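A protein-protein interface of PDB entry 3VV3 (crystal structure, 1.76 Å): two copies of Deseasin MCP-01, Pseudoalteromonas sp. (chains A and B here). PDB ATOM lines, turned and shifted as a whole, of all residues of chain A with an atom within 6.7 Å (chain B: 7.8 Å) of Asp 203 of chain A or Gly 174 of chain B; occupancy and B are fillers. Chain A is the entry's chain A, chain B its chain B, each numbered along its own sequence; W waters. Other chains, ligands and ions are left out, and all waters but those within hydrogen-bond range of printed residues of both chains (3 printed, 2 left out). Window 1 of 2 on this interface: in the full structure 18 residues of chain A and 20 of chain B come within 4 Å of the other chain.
The backbone carbonyl oxygen (O) of Asp 203 of chain A lies within hydrogen-bond range of the backbone NH (N) of Gly 176 of chain B (2.9 Å).
N of Gly 175 of chain B lies close to OD1 of Asp 203 of chain A (3.3 Å).
The backbone NH (N) of Asp 203 of chain A sits at hydrogen-bond distance from the backbone carbonyl oxygen (O) of Phe 237 of chain A, 3.3 Å away.
N of Asp 203 of chain A sits close to NE2 of Gln 239 of chain A, 2.9 Å away.
The backbone carbonyl oxygen (O) of Tyr 213 of chain B is in hydrogen-bond range of the backbone NH (N) of Gly 175 of chain B.
A ring nitrogen (ND1) of His 212 of chain B lies within hydrogen-bond range of the backbone carbonyl oxygen (O) of Ala 200 of chain B, 3.2 Å away.
The backbone NH (N) of Ala 204 of chain A lies within hydrogen-bond range of the backbone carbonyl oxygen (O) of Phe 237 of chain A, 2.9 Å away.
Water W2 lies within hydrogen-bond range of the backbone carbonyl oxygen (O) of Gly 176 of chain B (2.6 Å), the backbone NH (N) of Tyr 213 of chain B (3.0 Å) and the side-chain carboxylate (OD2) of Asp 203 of chain A (3.0 Å).
Water W1 bridges O of Asn 202 of chain A (2.7 Å) and O of Gly 174 of chain B (2.9 Å).
Water W3 bridges O of Ala 204 of chain A (3.1 Å) and N of Gly 177 of chain B (3.4 Å).
Among the printed residues, 5 pairs touch across the chains.
Among the printed residues, no Asp or Glu carboxylate lies within 4 Å of a Lys or Arg side-chain nitrogen of the other chain.
Positions printed for both chains: 200, 201, 202, 203 and 239.
Of chain B, only Gly 174 (3.7 Å), Gly 175 (3.0 Å), Gly 176 (2.9 Å) and His 212 (3.6 Å) come within 4 Å of Asp 203 of chain A.
Of chain A, only Asp 203 (3.7 Å) comes within 4 Å of Gly 174 of chain B.
Ala 204 of chain A touches just one residue of chain B: Gly 176.
Of the printed residues of chain A, Gly 175 of chain B touches Asp 203 (3.0 Å).
Of the printed residues of chain A, His 212 of chain B touches Asp 203.
Printed residues of chain A within 4 Å of Gly 176 of chain B: Asp 203 and Ala 204.
The nearest residue of chain B that does not touch Asp 203 of chain A is Tyr 213 of chain B (5.0 Å).
The nearest residue of chain A that does not touch Gly 174 of chain B is Asn 202 of chain A (4.5 Å).
The nearest printed residue of chain A that does not touch His 212 of chain B is Val 205 of chain A (7.4 Å).
Among the printed residues, merely in contact across the chains: Ala 204 of chain A with Gly 176 of chain B (3.5 Å), Asp 203 of chain A with His 212 of chain B (3.6 Å) and Asp 203 of chain A with Gly 174 of chain B (3.7 Å).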
ATOM      1  N   ALA A 200      11.531  18.528   8.372  1.00  0.00           N
ATOM      2  CA  ALA A 200      11.773  19.862   8.918  1.00  0.00           C
ATOM      3  C   ALA A 200      10.563  20.446   9.661  1.00  0.00           C
ATOM      4  O   ALA A 200      10.719  21.350  10.479  1.00  0.00           O
ATOM      5  CB  ALA A 200      12.247  20.824   7.823  1.00  0.00           C
ATOM      6  N   GLY A 201       9.367  19.934   9.379  1.00  0.00           N
ATOM      7  CA  GLY A 201       8.158  20.430  10.021  1.00  0.00           C
ATOM      8  C   GLY A 201       7.250  21.216   9.082  1.00  0.00           C
ATOM      9  O   GLY A 201       7.718  21.732   8.070  1.00  0.00           O
ATOM     10  N   ASN A 202       5.966  21.339   9.437  1.00  0.00           N
ATOM     11  CA  ASN A 202       4.975  21.921   8.525  1.00  0.00           C
ATOM     12  C   ASN A 202       4.372  23.244   8.982  1.00  0.00           C
ATOM     13  O   ASN A 202       3.245  23.576   8.614  1.00  0.00           O
ATOM     14  CB  ASN A 202       3.830  20.945   8.283  1.00  0.00           C
ATOM     15  CG  ASN A 202       4.304  19.612   7.763  1.00  0.00           C
ATOM     16  OD1 ASN A 202       5.367  19.518   7.169  1.00  0.00           O
ATOM     17  ND2 ASN A 202       3.511  18.571   7.988  1.00  0.00           N
ATOM     18  N   ASP A 203       5.126  24.002   9.761  1.00  0.00           N
ATOM     19  CA  ASP A 203       4.584  25.226  10.325  1.00  0.00           C
ATOM     20  C   ASP A 203       5.123  26.497   9.671  1.00  0.00           C
ATOM     21  O   ASP A 203       4.903  27.593  10.172  1.00  0.00           O
ATOM     22  CB  ASP A 203       4.804  25.265  11.840  1.00  0.00           C
ATOM     23  CG  ASP A 203       3.884  26.256  12.526  1.00  0.00           C
ATOM     24  OD1 ASP A 203       2.650  26.090  12.408  1.00  0.00           O
ATOM     25  OD2 ASP A 203       4.390  27.206  13.162  1.00  0.00           O
ATOM     26  N   ALA A 204       5.815  26.351   8.548  1.00  0.00           N
ATOM     27  CA  ALA A 204       6.193  27.512   7.737  1.00  0.00           C
ATOM     28  C   ALA A 204       6.923  28.602   8.524  1.00  0.00           C
ATOM     29  O   ALA A 204       6.585  29.786   8.428  1.00  0.00           O
ATOM     30  CB  ALA A 204       4.967  28.092   7.025  1.00  0.00           C
ATOM     31  N   VAL A 205       7.933  28.195   9.287  1.00  0.00           N
ATOM     32  CA  VAL A 205       8.797  29.132   9.997  1.00  0.00           C
ATOM     33  C   VAL A 205      10.263  28.736   9.863  1.00  0.00           C
ATOM     34  O   VAL A 205      10.588  27.633   9.413  1.00  0.00           O
ATOM     35  CB  VAL A 205       8.443  29.235  11.492  1.00  0.00           C
ATOM     36  CG1 VAL A 205       7.040  29.828  11.666  1.00  0.00           C
ATOM     37  CG2 VAL A 205       8.564  27.873  12.169  1.00  0.00           C
ATOM     38  N   ASP A 206      11.130  29.656  10.271  1.00  0.00           N
ATOM     39  CA  ASP A 206      12.581  29.495  10.203  1.00  0.00           C
ATOM     40  C   ASP A 206      13.103  28.699  11.398  1.00  0.00           C
ATOM     41  O   ASP A 206      13.030  29.160  12.540  1.00  0.00           O
ATOM     42  CB  ASP A 206      13.210  30.894  10.151  1.00  0.00           C
ATOM     43  CG  ASP A 206      14.719  30.877  10.282  1.00  0.00           C
ATOM     44  OD1 ASP A 206      15.337  29.808  10.093  1.00  0.00           O
ATOM     45  OD2 ASP A 206      15.287  31.956  10.571  1.00  0.00           O
ATOM     46  N   SER A 236       4.352  25.660   0.582  1.00  0.00           N
ATOM     47  CA  SER A 236       3.975  26.796   1.425  1.00  0.00           C
ATOM     48  C   SER A 236       4.010  26.489   2.922  1.00  0.00           C
ATOM     49  O   SER A 236       4.306  27.374   3.720  1.00  0.00           O
ATOM     50  CB  SER A 236       2.616  27.375   1.019  1.00  0.00           C
ATOM     51  OG  SER A 236       1.654  26.351   0.885  1.00  0.00           O
ATOM     52  N   PHE A 237       3.716  25.242   3.289  1.00  0.00           N
ATOM     53  CA  PHE A 237       3.727  24.821   4.689  1.00  0.00           C
ATOM     54  C   PHE A 237       5.115  24.519   5.252  1.00  0.00           C
ATOM     55  O   PHE A 237       5.275  24.408   6.463  1.00  0.00           O
ATOM     56  CB  PHE A 237       2.832  23.588   4.889  1.00  0.00           C
ATOM     57  CG  PHE A 237       3.191  22.426   3.995  1.00  0.00           C
ATOM     58  CD1 PHE A 237       4.284  21.628   4.286  1.00  0.00           C
ATOM     59  CD2 PHE A 237       2.430  22.138   2.870  1.00  0.00           C
ATOM     60  CE1 PHE A 237       4.632  20.563   3.465  1.00  0.00           C
ATOM     61  CE2 PHE A 237       2.764  21.057   2.032  1.00  0.00           C
ATOM     62  CZ  PHE A 237       3.869  20.272   2.334  1.00  0.00           C
ATOM     63  N   SER A 238       6.121  24.385   4.394  1.00  0.00           N
ATOM     64  CA  SER A 238       7.405  23.848   4.856  1.00  0.00           C
ATOM     65  C   SER A 238       8.175  24.774   5.787  1.00  0.00           C
ATOM     66  O   SER A 238       8.290  25.965   5.536  1.00  0.00           O
ATOM     67  CB  SER A 238       8.308  23.483   3.672  1.00  0.00           C
ATOM     68  OG  SER A 238       9.463  22.767   4.116  1.00  0.00           O
ATOM     69  N   GLN A 239       8.739  24.204   6.841  1.00  0.00           N
ATOM     70  CA  GLN A 239       9.736  24.920   7.625  1.00  0.00           C
ATOM     71  C   GLN A 239      11.054  24.903   6.842  1.00  0.00           C
ATOM     72  O   GLN A 239      11.199  24.153   5.871  1.00  0.00           O
ATOM     73  CB  GLN A 239       9.860  24.299   9.028  1.00  0.00           C
ATOM     74  CG  GLN A 239       8.701  24.742   9.943  1.00  0.00           C
ATOM     75  CD  GLN A 239       8.547  23.913  11.204  1.00  0.00           C
ATOM     76  OE1 GLN A 239       9.437  23.866  12.066  1.00  0.00           O
ATOM     77  NE2 GLN A 239       7.400  23.274  11.333  1.00  0.00           N
ATOM     78  N   TRP A 240      11.989  25.760   7.230  1.00  0.00           N
ATOM     79  CA  TRP A 240      13.273  25.851   6.540  1.00  0.00           C
ATOM     80  C   TRP A 240      14.320  26.230   7.577  1.00  0.00           C
ATOM     81  O   TRP A 240      14.006  26.349   8.757  1.00  0.00           O
ATOM     82  CB  TRP A 240      13.220  26.892   5.409  1.00  0.00           C
ATOM     83  CG  TRP A 240      13.007  28.295   5.908  1.00  0.00           C
ATOM     84  CD1 TRP A 240      13.973  29.202   6.254  1.00  0.00           C
ATOM     85  CD2 TRP A 240      11.749  28.937   6.149  1.00  0.00           C
ATOM     86  NE1 TRP A 240      13.391  30.373   6.688  1.00  0.00           N
ATOM     87  CE2 TRP A 240      12.027  30.235   6.629  1.00  0.00           C
ATOM     88  CE3 TRP A 240      10.416  28.544   5.995  1.00  0.00           C
ATOM     89  CZ2 TRP A 240      11.017  31.139   6.961  1.00  0.00           C
ATOM     90  CZ3 TRP A 240       9.413  29.451   6.327  1.00  0.00           C
ATOM     91  CH2 TRP A 240       9.722  30.728   6.801  1.00  0.00           C
ATOM     92  N   PHE B 137      -9.044  27.340   1.226  1.00  0.00           N
ATOM     93  CA  PHE B 137      -7.841  28.128   0.956  1.00  0.00           C
ATOM     94  C   PHE B 137      -6.615  27.241   0.836  1.00  0.00           C
ATOM     95  O   PHE B 137      -5.554  27.716   0.463  1.00  0.00           O
ATOM     96  CB  PHE B 137      -7.601  29.264   1.975  1.00  0.00           C
ATOM     97  CG  PHE B 137      -6.923  28.824   3.254  1.00  0.00           C
ATOM     98  CD1 PHE B 137      -7.608  28.072   4.193  1.00  0.00           C
ATOM     99  CD2 PHE B 137      -5.603  29.192   3.521  1.00  0.00           C
ATOM    100  CE1 PHE B 137      -6.989  27.673   5.377  1.00  0.00           C
ATOM    101  CE2 PHE B 137      -4.973  28.800   4.709  1.00  0.00           C
ATOM    102  CZ  PHE B 137      -5.672  28.045   5.635  1.00  0.00           C
ATOM    103  N   LEU B 138      -6.778  25.948   1.127  1.00  0.00           N
ATOM    104  CA  LEU B 138      -5.671  24.999   0.995  1.00  0.00           C
ATOM    105  C   LEU B 138      -5.961  24.058  -0.157  1.00  0.00           C
ATOM    106  O   LEU B 138      -7.045  23.469  -0.226  1.00  0.00           O
ATOM    107  CB  LEU B 138      -5.468  24.191   2.277  1.00  0.00           C
ATOM    108  CG  LEU B 138      -4.998  24.991   3.496  1.00  0.00           C
ATOM    109  CD1 LEU B 138      -5.230  24.212   4.785  1.00  0.00           C
ATOM    110  CD2 LEU B 138      -3.535  25.421   3.349  1.00  0.00           C
ATOM    111  N   ASN B 171     -11.085  26.781  12.463  1.00  0.00           N
ATOM    112  CA  ASN B 171      -9.777  26.968  11.842  1.00  0.00           C
ATOM    113  C   ASN B 171      -8.782  25.915  12.310  1.00  0.00           C
ATOM    114  O   ASN B 171      -7.976  26.153  13.214  1.00  0.00           O
ATOM    115  CB  ASN B 171      -9.251  28.369  12.131  1.00  0.00           C
ATOM    116  CG  ASN B 171     -10.196  29.442  11.637  1.00  0.00           C
ATOM    117  OD1 ASN B 171     -10.120  29.865  10.481  1.00  0.00           O
ATOM    118  ND2 ASN B 171     -11.115  29.866  12.499  1.00  0.00           N
ATOM    119  N   SER B 172      -8.866  24.744  11.691  1.00  0.00           N
ATOM    120  CA  SER B 172      -7.996  23.620  11.999  1.00  0.00           C
ATOM    121  C   SER B 172      -6.766  23.683  11.109  1.00  0.00           C
ATOM    122  O   SER B 172      -6.533  22.808  10.274  1.00  0.00           O
ATOM    123  CB  SER B 172      -8.753  22.319  11.758  1.00  0.00           C
ATOM    124  OG  SER B 172      -9.729  22.126  12.769  1.00  0.00           O
ATOM    125  N   TRP B 173      -6.001  24.753  11.273  1.00  0.00           N
ATOM    126  CA  TRP B 173      -4.804  24.982  10.476  1.00  0.00           C
ATOM    127  C   TRP B 173      -3.907  25.946  11.243  1.00  0.00           C
ATOM    128  O   TRP B 173      -4.335  26.563  12.210  1.00  0.00           O
ATOM    129  CB  TRP B 173      -5.163  25.542   9.090  1.00  0.00           C
ATOM    130  CG  TRP B 173      -5.998  26.803   9.109  1.00  0.00           C
ATOM    131  CD1 TRP B 173      -7.364  26.892   9.066  1.00  0.00           C
ATOM    132  CD2 TRP B 173      -5.512  28.150   9.166  1.00  0.00           C
ATOM    133  NE1 TRP B 173      -7.753  28.213   9.106  1.00  0.00           N
ATOM    134  CE2 TRP B 173      -6.634  29.003   9.163  1.00  0.00           C
ATOM    135  CE3 TRP B 173      -4.235  28.716   9.216  1.00  0.00           C
ATOM    136  CZ2 TRP B 173      -6.518  30.389   9.215  1.00  0.00           C
ATOM    137  CZ3 TRP B 173      -4.125  30.096   9.266  1.00  0.00           C
ATOM    138  CH2 TRP B 173      -5.256  30.913   9.269  1.00  0.00           C
ATOM    139  N   GLY B 174      -2.655  26.055  10.826  1.00  0.00           N
ATOM    140  CA  GLY B 174      -1.743  26.986  11.454  1.00  0.00           C
ATOM    141  C   GLY B 174      -0.448  27.024  10.681  1.00  0.00           C
ATOM    142  O   GLY B 174      -0.214  26.184   9.810  1.00  0.00           O
ATOM    143  N   GLY B 175       0.388  28.002  11.003  1.00  0.00           N
ATOM    144  CA  GLY B 175       1.700  28.126  10.398  1.00  0.00           C
ATOM    145  C   GLY B 175       1.969  29.565  10.040  1.00  0.00           C
ATOM    146  O   GLY B 175       1.039  30.365   9.931  1.00  0.00           O
ATOM    147  N   GLY B 176       3.242  29.901   9.867  1.00  0.00           N
ATOM    148  CA  GLY B 176       3.628  31.242   9.475  1.00  0.00           C
ATOM    149  C   GLY B 176       3.833  32.156  10.665  1.00  0.00           C
ATOM    150  O   GLY B 176       3.520  31.809  11.800  1.00  0.00           O
ATOM    151  N   GLY B 177       4.383  33.334  10.410  1.00  0.00           N
ATOM    152  CA  GLY B 177       4.581  34.290  11.475  1.00  0.00           C
ATOM    153  C   GLY B 177       3.346  35.152  11.616  1.00  0.00           C
ATOM    154  O   GLY B 177       2.388  35.006  10.852  1.00  0.00           O
ATOM    155  N   ALA B 198      -9.579  27.907  16.960  1.00  0.00           N
ATOM    156  CA  ALA B 198      -8.277  27.648  16.339  1.00  0.00           C
ATOM    157  C   ALA B 198      -7.537  26.516  17.039  1.00  0.00           C
ATOM    158  O   ALA B 198      -7.610  26.387  18.254  1.00  0.00           O
ATOM    159  CB  ALA B 198      -7.428  28.912  16.365  1.00  0.00           C
ATOM    160  N   ALA B 199      -6.813  25.716  16.262  1.00  0.00           N
ATOM    161  CA  ALA B 199      -6.035  24.593  16.787  1.00  0.00           C
ATOM    162  C   ALA B 199      -4.712  25.060  17.393  1.00  0.00           C
ATOM    163  O   ALA B 199      -4.018  25.900  16.812  1.00  0.00           O
ATOM    164  CB  ALA B 199      -5.764  23.607  15.663  1.00  0.00           C
ATOM    165  N   ALA B 200      -4.346  24.503  18.546  1.00  0.00           N
ATOM    166  CA  ALA B 200      -3.112  24.913  19.211  1.00  0.00           C
ATOM    167  C   ALA B 200      -1.830  24.427  18.528  1.00  0.00           C
ATOM    168  O   ALA B 200      -0.771  25.027  18.706  1.00  0.00           O
ATOM    169  CB  ALA B 200      -3.120  24.490  20.680  1.00  0.00           C
ATOM    170  N   GLY B 201      -1.911  23.335  17.767  1.00  0.00           N
ATOM    171  CA  GLY B 201      -0.726  22.794  17.113  1.00  0.00           C
ATOM    172  C   GLY B 201      -0.279  21.454  17.676  1.00  0.00           C
ATOM    173  O   GLY B 201      -0.596  21.139  18.824  1.00  0.00           O
ATOM    174  N   ASN B 202       0.468  20.684  16.876  1.00  0.00           N
ATOM    175  CA  ASN B 202       0.811  19.286  17.207  1.00  0.00           C
ATOM    176  C   ASN B 202       2.283  19.018  17.493  1.00  0.00           C
ATOM    177  O   ASN B 202       2.762  17.895  17.323  1.00  0.00           O
ATOM    178  CB  ASN B 202       0.377  18.361  16.066  1.00  0.00           C
ATOM    179  CG  ASN B 202      -1.099  18.459  15.769  1.00  0.00           C
ATOM    180  OD1 ASN B 202      -1.890  18.848  16.626  1.00  0.00           O
ATOM    181  ND2 ASN B 202      -1.482  18.096  14.555  1.00  0.00           N
ATOM    182  N   ASP B 203       3.009  20.031  17.942  1.00  0.00           N
ATOM    183  CA  ASP B 203       4.451  19.878  18.091  1.00  0.00           C
ATOM    184  C   ASP B 203       4.906  19.750  19.546  1.00  0.00           C
ATOM    185  O   ASP B 203       6.098  19.825  19.822  1.00  0.00           O
ATOM    186  CB  ASP B 203       5.173  21.042  17.397  1.00  0.00           C
ATOM    187  CG  ASP B 203       6.635  20.734  17.082  1.00  0.00           C
ATOM    188  OD1 ASP B 203       6.921  19.643  16.540  1.00  0.00           O
ATOM    189  OD2 ASP B 203       7.497  21.595  17.358  1.00  0.00           O
ATOM    190  N   ASN B 210       6.677  30.051  22.562  1.00  0.00           N
ATOM    191  CA  ASN B 210       6.838  29.721  21.151  1.00  0.00           C
ATOM    192  C   ASN B 210       5.524  29.967  20.403  1.00  0.00           C
ATOM    193  O   ASN B 210       4.756  29.038  20.192  1.00  0.00           O
ATOM    194  CB  ASN B 210       7.207  28.237  21.001  1.00  0.00           C
ATOM    195  CG  ASN B 210       8.439  27.842  21.807  1.00  0.00           C
ATOM    196  OD1 ASN B 210       9.570  28.186  21.447  1.00  0.00           O
ATOM    197  ND2 ASN B 210       8.226  27.097  22.896  1.00  0.00           N
ATOM    198  N   PRO B 211       5.261  31.222  20.009  1.00  0.00           N
ATOM    199  CA  PRO B 211       3.954  31.556  19.430  1.00  0.00           C
ATOM    200  C   PRO B 211       3.656  30.779  18.157  1.00  0.00           C
ATOM    201  O   PRO B 211       4.535  30.604  17.318  1.00  0.00           O
ATOM    202  CB  PRO B 211       4.073  33.051  19.120  1.00  0.00           C
ATOM    203  CG  PRO B 211       5.157  33.542  20.027  1.00  0.00           C
ATOM    204  CD  PRO B 211       6.129  32.404  20.133  1.00  0.00           C
ATOM    205  N   HIS B 212       2.405  30.344  18.039  1.00  0.00           N
ATOM    206  CA  HIS B 212       1.899  29.565  16.920  1.00  0.00           C
ATOM    207  C   HIS B 212       0.683  30.326  16.404  1.00  0.00           C
ATOM    208  O   HIS B 212      -0.152  30.757  17.203  1.00  0.00           O
ATOM    209  CB  HIS B 212       1.506  28.180  17.465  1.00  0.00           C
ATOM    210  CG  HIS B 212       0.724  27.320  16.519  1.00  0.00           C
ATOM    211  ND1 HIS B 212      -0.654  27.335  16.462  1.00  0.00           N
ATOM    212  CD2 HIS B 212       1.123  26.357  15.650  1.00  0.00           C
ATOM    213  CE1 HIS B 212      -1.068  26.451  15.569  1.00  0.00           C
ATOM    214  NE2 HIS B 212      -0.009  25.845  15.064  1.00  0.00           N
ATOM    215  N   TYR B 213       0.582  30.521  15.089  1.00  0.00           N
ATOM    216  CA  TYR B 213      -0.553  31.266  14.531  1.00  0.00           C
ATOM    217  C   TYR B 213      -1.438  30.405  13.637  1.00  0.00           C
ATOM    218  O   TYR B 213      -0.940  29.526  12.943  1.00  0.00           O
ATOM    219  CB  TYR B 213      -0.071  32.521  13.792  1.00  0.00           C
ATOM    220  CG  TYR B 213       0.612  33.475  14.731  1.00  0.00           C
ATOM    221  CD1 TYR B 213      -0.131  34.349  15.528  1.00  0.00           C
ATOM    222  CD2 TYR B 213       1.994  33.472  14.865  1.00  0.00           C
ATOM    223  CE1 TYR B 213       0.491  35.213  16.410  1.00  0.00           C
ATOM    224  CE2 TYR B 213       2.628  34.324  15.759  1.00  0.00           C
ATOM    225  CZ  TYR B 213       1.873  35.189  16.521  1.00  0.00           C
ATOM    226  OH  TYR B 213       2.504  36.038  17.402  1.00  0.00           O
ATOM    227  N   PRO B 214      -2.756  30.672  13.641  1.00  0.00           N
ATOM    228  CA  PRO B 214      -3.433  31.800  14.303  1.00  0.00           C
ATOM    229  C   PRO B 214      -3.794  31.611  15.786  1.00  0.00           C
ATOM    230  O   PRO B 214      -4.408  32.511  16.364  1.00  0.00           O
ATOM    231  CB  PRO B 214      -4.725  31.948  13.485  1.00  0.00           C
ATOM    232  CG  PRO B 214      -5.028  30.520  13.053  1.00  0.00           C
ATOM    233  CD  PRO B 214      -3.683  29.871  12.819  1.00  0.00           C
ATOM    234  N   SER B 215      -3.424  30.482  16.389  1.00  0.00           N
ATOM    235  CA  SER B 215      -3.769  30.194  17.782  1.00  0.00           C
ATOM    236  C   SER B 215      -3.383  31.327  18.748  1.00  0.00           C
ATOM    237  O   SER B 215      -4.147  31.672  19.662  1.00  0.00           O
ATOM    238  CB  SER B 215      -3.072  28.890  18.224  1.00  0.00           C
ATOM    239  OG  SER B 215      -3.488  28.519  19.525  1.00  0.00           O
ATOM    240  N   GLN B 239       0.316  20.945  21.532  1.00  0.00           N
ATOM    241  CA  GLN B 239       0.893  22.164  22.068  1.00  0.00           C
ATOM    242  C   GLN B 239       0.008  22.685  23.195  1.00  0.00           C
ATOM    243  O   GLN B 239      -1.160  22.298  23.310  1.00  0.00           O
ATOM    244  CB  GLN B 239       1.094  23.202  20.958  1.00  0.00           C
ATOM    245  CG  GLN B 239       2.335  22.866  20.130  1.00  0.00           C
ATOM    246  CD  GLN B 239       2.416  23.576  18.791  1.00  0.00           C
ATOM    247  OE1 GLN B 239       2.485  24.812  18.718  1.00  0.00           O
ATOM    248  NE2 GLN B 239       2.450  22.791  17.721  1.00  0.00           N
ATOM    249  N   SER B 270      -6.219  19.683  15.174  1.00  0.00           N
ATOM    250  CA  SER B 270      -7.175  19.938  14.087  1.00  0.00           C
ATOM    251  C   SER B 270      -8.485  19.187  14.257  1.00  0.00           C
ATOM    252  O   SER B 270      -9.509  19.592  13.710  1.00  0.00           O
ATOM    253  CB  SER B 270      -6.576  19.590  12.726  1.00  0.00           C
ATOM    254  OG  SER B 270      -5.574  20.529  12.368  1.00  0.00           O
HETATM  255  O   HOH W   1       1.757  25.658   7.765  1.00  0.00           O
HETATM  256  O   HOH W   2       2.890  29.782  13.346  1.00  0.00           O
HETATM  257  O   HOH W   3       7.505  32.709   9.140  1.00  0.00           O
